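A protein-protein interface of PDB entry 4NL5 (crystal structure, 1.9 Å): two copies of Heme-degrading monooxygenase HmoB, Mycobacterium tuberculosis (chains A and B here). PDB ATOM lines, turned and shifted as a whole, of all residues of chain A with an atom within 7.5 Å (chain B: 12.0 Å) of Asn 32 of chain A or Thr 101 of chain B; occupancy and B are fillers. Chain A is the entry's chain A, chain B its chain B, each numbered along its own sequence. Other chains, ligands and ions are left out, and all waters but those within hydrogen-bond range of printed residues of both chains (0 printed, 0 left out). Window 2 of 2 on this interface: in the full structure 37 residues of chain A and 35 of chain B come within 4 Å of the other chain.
Of the 5 printed residues of chain B, 4 touch a printed residue of chain A.
Of the 13 printed residues of chain A, 7 touch a printed residue of chain B.
Printed residues of chain A that touch a printed residue of chain B: Ala 27, His 28, Glu 31, Asn 32, Phe 36, Leu 37 and Gly 38.
Hydrophobic or aromatic side chains of chain A within 4 Å of the printed part of chain B: Ala 27, His 28 and Phe 36.
Among the printed residues, no Asp or Glu carboxylate lies within 4 Å of a Lys or Arg side-chain nitrogen of the other chain.
Of the printed residues of chain B, Ala 27 of chain A touches Val 98 (3.98 Å).
Printed residues of chain B within 4 Å of His 28 of chain A: Val 98.
No residue of chain B comes within 4 Å of Ala 29 of chain A.
No residue of chain B comes within 4 Å of Val 30 of chain A.
Asn 32 of chain A touches just one residue of chain B: Thr 101 (3.2 Å).
No residue of chain B comes within 4 Å of Ser 33 of chain A.
No residue of chain B comes within 4 Å of Pro 34 of chain A.
Phe 36 of chain A touches one residue of chain B.
Of the printed residues of chain B, Leu 37 of chain A touches Gly 100 (3.5 Å).
Of the printed residues of chain A, Val 98 of chain B touches Ala 27, His 28 and Gly 38.
Of the printed residues of chain A, Gly 99 of chain B touches Glu 31 and Gly 38.
Of chain A, only Glu 31 (3.5 Å), Phe 36 (3.8 Å), Leu 37 (3.5 Å) and Gly 38 (3.7 Å) come within 4 Å of Gly 100 of chain B.
Of chain A, only Glu 31 (3.0 Å) and Asn 32 (3.2 Å) come within 4 Å of Thr 101 of chain B.
The nearest residue of chain B that does not touch Asn 32 of chain A is Gly 100 of chain B (5.5 Å).
The nearest residue of chain A that does not touch Thr 101 of chain B is Phe 36 of chain A (5.4 Å).
A ring nitrogen (ND1) of His 28 of chain A is in hydrogen-bond range of the side-chain carboxylate (OE1) of Glu 31 of chain A, at 2.8 Å.
No position is printed for both chains.
Of the 11 pairs that touch across the chains among the printed residues, none has its exchanged pair printed and touching as well.
Among the printed residues, pairs that only touch across the chains: Gly 38 of chain A with Val 98 of chain B, Asn 32 of chain A with Thr 101 of chain B, Glu 31 of chain A with Gly 100 of chain B, Glu 31 of chain A with Gly 99 of chain B, Gly 38 of chain A with Gly 100 of chain B, Phe 36 of chain A with Gly 100 of chain B, His 28 of chain A with Val 98 of chain B, Gly 38 of chain A with Gly 99 of chain B and Ala 27 of chain A with Val 98 of chain B.
N of Thr 101 of chain B is in hydrogen-bond range of O of Glu 31 of chain A.
The backbone NH (N) of Gly 100 of chain B sits at hydrogen-bond distance from the backbone carbonyl oxygen (O) of Leu 37 of chain A, 3.5 Å away.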
ATOM      1  N   ALA A  27     -20.332  -3.951 -11.720  1.00  0.00           N
ATOM      2  CA  ALA A  27     -20.286  -4.636 -10.427  1.00  0.00           C
ATOM      3  C   ALA A  27     -20.731  -6.090 -10.515  1.00  0.00           C
ATOM      4  O   ALA A  27     -20.244  -6.950  -9.771  1.00  0.00           O
ATOM      5  CB  ALA A  27     -21.138  -3.903  -9.405  1.00  0.00           C
ATOM      6  N   HIS A  28     -21.655  -6.366 -11.428  1.00  0.00           N
ATOM      7  CA  HIS A  28     -22.280  -7.677 -11.469  1.00  0.00           C
ATOM      8  C   HIS A  28     -21.777  -8.509 -12.643  1.00  0.00           C
ATOM      9  O   HIS A  28     -22.486  -9.378 -13.149  1.00  0.00           O
ATOM     10  CB  HIS A  28     -23.801  -7.515 -11.531  1.00  0.00           C
ATOM     11  CG  HIS A  28     -24.371  -6.766 -10.364  1.00  0.00           C
ATOM     12  ND1 HIS A  28     -24.429  -7.291  -9.091  1.00  0.00           N
ATOM     13  CD2 HIS A  28     -24.903  -5.523 -10.281  1.00  0.00           C
ATOM     14  CE1 HIS A  28     -24.974  -6.405  -8.275  1.00  0.00           C
ATOM     15  NE2 HIS A  28     -25.269  -5.324  -8.973  1.00  0.00           N
ATOM     16  N   ALA A  29     -20.546  -8.245 -13.067  1.00  0.00           N
ATOM     17  CA  ALA A  29     -19.926  -9.035 -14.120  1.00  0.00           C
ATOM     18  C   ALA A  29     -19.210 -10.237 -13.516  1.00  0.00           C
ATOM     19  O   ALA A  29     -19.047 -11.274 -14.160  1.00  0.00           O
ATOM     20  CB  ALA A  29     -18.963  -8.181 -14.924  1.00  0.00           C
ATOM     21  N   VAL A  30     -18.775 -10.074 -12.271  1.00  0.00           N
ATOM     22  CA  VAL A  30     -18.016 -11.094 -11.572  1.00  0.00           C
ATOM     23  C   VAL A  30     -18.908 -11.858 -10.609  1.00  0.00           C
ATOM     24  O   VAL A  30     -18.491 -12.847 -10.018  1.00  0.00           O
ATOM     25  CB  VAL A  30     -16.846 -10.443 -10.780  1.00  0.00           C
ATOM     26  CG1 VAL A  30     -15.869 -11.489 -10.239  1.00  0.00           C
ATOM     27  CG2 VAL A  30     -16.124  -9.428 -11.654  1.00  0.00           C
ATOM     28  N   GLU A  31     -20.169 -11.448 -10.536  1.00  0.00           N
ATOM     29  CA  GLU A  31     -21.079 -11.922  -9.492  1.00  0.00           C
ATOM     30  C   GLU A  31     -21.247 -13.436  -9.346  1.00  0.00           C
ATOM     31  O   GLU A  31     -21.129 -13.959  -8.234  1.00  0.00           O
ATOM     32  CB  GLU A  31     -22.459 -11.295  -9.701  1.00  0.00           C
ATOM     33  CG  GLU A  31     -23.255 -11.175  -8.420  1.00  0.00           C
ATOM     34  CD  GLU A  31     -24.433 -10.234  -8.547  1.00  0.00           C
ATOM     35  OE1 GLU A  31     -24.895  -9.999  -9.684  1.00  0.00           O
ATOM     36  OE2 GLU A  31     -24.888  -9.713  -7.507  1.00  0.00           O
ATOM     37  N   ASN A  32     -21.515 -14.130 -10.447  1.00  0.00           N
ATOM     38  CA  ASN A  32     -21.631 -15.585 -10.431  1.00  0.00           C
ATOM     39  C   ASN A  32     -20.353 -16.395 -10.650  1.00  0.00           C
ATOM     40  O   ASN A  32     -20.428 -17.583 -10.961  1.00  0.00           O
ATOM     41  CB  ASN A  32     -22.677 -16.047 -11.458  1.00  0.00           C
ATOM     42  CG  ASN A  32     -24.096 -15.978 -10.921  1.00  0.00           C
ATOM     43  OD1 ASN A  32     -24.348 -15.397  -9.864  1.00  0.00           O
ATOM     44  ND2 ASN A  32     -25.032 -16.588 -11.641  1.00  0.00           N
ATOM     45  N   SER A  33     -19.186 -15.781 -10.491  1.00  0.00           N
ATOM     46  CA  SER A  33     -17.938 -16.519 -10.695  1.00  0.00           C
ATOM     47  C   SER A  33     -17.757 -17.590  -9.618  1.00  0.00           C
ATOM     48  O   SER A  33     -18.068 -17.369  -8.453  1.00  0.00           O
ATOM     49  CB  SER A  33     -16.737 -15.573 -10.706  1.00  0.00           C
ATOM     50  OG  SER A  33     -16.826 -14.672 -11.794  1.00  0.00           O
ATOM     51  N   PRO A  34     -17.317 -18.788 -10.023  1.00  0.00           N
ATOM     52  CA  PRO A  34     -17.162 -19.870  -9.041  1.00  0.00           C
ATOM     53  C   PRO A  34     -16.177 -19.511  -7.933  1.00  0.00           C
ATOM     54  O   PRO A  34     -15.067 -19.047  -8.196  1.00  0.00           O
ATOM     55  CB  PRO A  34     -16.635 -21.034  -9.886  1.00  0.00           C
ATOM     56  CG  PRO A  34     -17.103 -20.735 -11.258  1.00  0.00           C
ATOM     57  CD  PRO A  34     -17.019 -19.238 -11.389  1.00  0.00           C
ATOM     58  N   GLY A  35     -16.603 -19.694  -6.690  1.00  0.00           N
ATOM     59  CA  GLY A  35     -15.746 -19.413  -5.552  1.00  0.00           C
ATOM     60  C   GLY A  35     -15.717 -17.940  -5.177  1.00  0.00           C
ATOM     61  O   GLY A  35     -15.101 -17.555  -4.182  1.00  0.00           O
ATOM     62  N   PHE A  36     -16.368 -17.099  -5.973  1.00  0.00           N
ATOM     63  CA  PHE A  36     -16.353 -15.662  -5.682  1.00  0.00           C
ATOM     64  C   PHE A  36     -17.278 -15.368  -4.510  1.00  0.00           C
ATOM     65  O   PHE A  36     -18.434 -15.777  -4.517  1.00  0.00           O
ATOM     66  CB  PHE A  36     -16.780 -14.847  -6.907  1.00  0.00           C
ATOM     67  CG  PHE A  36     -16.746 -13.359  -6.688  1.00  0.00           C
ATOM     68  CD1 PHE A  36     -15.562 -12.719  -6.359  1.00  0.00           C
ATOM     69  CD2 PHE A  36     -17.901 -12.605  -6.803  1.00  0.00           C
ATOM     70  CE1 PHE A  36     -15.524 -11.337  -6.161  1.00  0.00           C
ATOM     71  CE2 PHE A  36     -17.870 -11.228  -6.607  1.00  0.00           C
ATOM     72  CZ  PHE A  36     -16.682 -10.604  -6.287  1.00  0.00           C
ATOM     73  N   LEU A  37     -16.775 -14.658  -3.504  1.00  0.00           N
ATOM     74  CA  LEU A  37     -17.580 -14.387  -2.310  1.00  0.00           C
ATOM     75  C   LEU A  37     -18.027 -12.934  -2.217  1.00  0.00           C
ATOM     76  O   LEU A  37     -18.824 -12.573  -1.354  1.00  0.00           O
ATOM     77  CB  LEU A  37     -16.801 -14.762  -1.050  1.00  0.00           C
ATOM     78  CG  LEU A  37     -16.458 -16.247  -0.910  1.00  0.00           C
ATOM     79  CD1 LEU A  37     -15.701 -16.488   0.403  1.00  0.00           C
ATOM     80  CD2 LEU A  37     -17.734 -17.066  -0.953  1.00  0.00           C
ATOM     81  N   GLY A  38     -17.572 -12.109  -3.145  1.00  0.00           N
ATOM     82  CA  GLY A  38     -17.991 -10.722  -3.155  1.00  0.00           C
ATOM     83  C   GLY A  38     -16.835  -9.747  -3.121  1.00  0.00           C
ATOM     84  O   GLY A  38     -15.672 -10.132  -2.981  1.00  0.00           O
ATOM     85  N   TRP A  66     -10.350 -17.635 -12.230  1.00  0.00           N
ATOM     86  CA  TRP A  66     -11.038 -16.442 -12.704  1.00  0.00           C
ATOM     87  C   TRP A  66     -10.080 -15.521 -13.447  1.00  0.00           C
ATOM     88  O   TRP A  66     -10.429 -14.954 -14.483  1.00  0.00           O
ATOM     89  CB  TRP A  66     -11.695 -15.709 -11.520  1.00  0.00           C
ATOM     90  CG  TRP A  66     -12.380 -14.414 -11.904  1.00  0.00           C
ATOM     91  CD1 TRP A  66     -13.591 -14.270 -12.532  1.00  0.00           C
ATOM     92  CD2 TRP A  66     -11.888 -13.091 -11.674  1.00  0.00           C
ATOM     93  NE1 TRP A  66     -13.878 -12.932 -12.704  1.00  0.00           N
ATOM     94  CE2 TRP A  66     -12.846 -12.190 -12.193  1.00  0.00           C
ATOM     95  CE3 TRP A  66     -10.733 -12.578 -11.075  1.00  0.00           C
ATOM     96  CZ2 TRP A  66     -12.681 -10.806 -12.127  1.00  0.00           C
ATOM     97  CZ3 TRP A  66     -10.570 -11.201 -11.024  1.00  0.00           C
ATOM     98  CH2 TRP A  66     -11.538 -10.335 -11.548  1.00  0.00           C
ATOM     99  N   ASP B  97     -20.486  -2.419  -2.217  1.00  0.00           N
ATOM    100  CA  ASP B  97     -20.378  -3.655  -1.452  1.00  0.00           C
ATOM    101  C   ASP B  97     -21.272  -4.685  -2.122  1.00  0.00           C
ATOM    102  O   ASP B  97     -22.496  -4.622  -2.015  1.00  0.00           O
ATOM    103  CB  ASP B  97     -20.787  -3.435   0.005  1.00  0.00           C
ATOM    104  CG  ASP B  97     -20.363  -4.578   0.912  1.00  0.00           C
ATOM    105  OD1 ASP B  97     -20.021  -5.662   0.390  1.00  0.00           O
ATOM    106  OD2 ASP B  97     -20.391  -4.398   2.148  1.00  0.00           O
ATOM    107  N   VAL B  98     -20.658  -5.623  -2.829  1.00  0.00           N
ATOM    108  CA  VAL B  98     -21.410  -6.532  -3.678  1.00  0.00           C
ATOM    109  C   VAL B  98     -21.135  -7.972  -3.283  1.00  0.00           C
ATOM    110  O   VAL B  98     -19.981  -8.377  -3.222  1.00  0.00           O
ATOM    111  CB  VAL B  98     -21.022  -6.346  -5.149  1.00  0.00           C
ATOM    112  CG1 VAL B  98     -21.878  -7.224  -6.036  1.00  0.00           C
ATOM    113  CG2 VAL B  98     -21.133  -4.872  -5.548  1.00  0.00           C
ATOM    114  N   GLY B  99     -22.184  -8.749  -3.037  1.00  0.00           N
ATOM    115  CA  GLY B  99     -22.016 -10.152  -2.696  1.00  0.00           C
ATOM    116  C   GLY B  99     -21.818 -11.030  -3.923  1.00  0.00           C
ATOM    117  O   GLY B  99     -22.099 -10.608  -5.042  1.00  0.00           O
ATOM    118  N   GLY B 100     -21.336 -12.252  -3.716  1.00  0.00           N
ATOM    119  CA  GLY B 100     -21.243 -13.217  -4.799  1.00  0.00           C
ATOM    120  C   GLY B 100     -22.534 -14.009  -4.903  1.00  0.00           C
ATOM    121  O   GLY B 100     -22.916 -14.699  -3.959  1.00  0.00           O
ATOM    122  N   THR B 101     -23.211 -13.910  -6.043  1.00  0.00           N
ATOM    123  CA  THR B 101     -24.504 -14.565  -6.223  1.00  0.00           C
ATOM    124  C   THR B 101     -24.337 -16.028  -6.610  1.00  0.00           C
ATOM    125  O   THR B 101     -23.855 -16.834  -5.816  1.00  0.00           O
ATOM    126  CB  THR B 101     -25.330 -13.831  -7.271  1.00  0.00           C
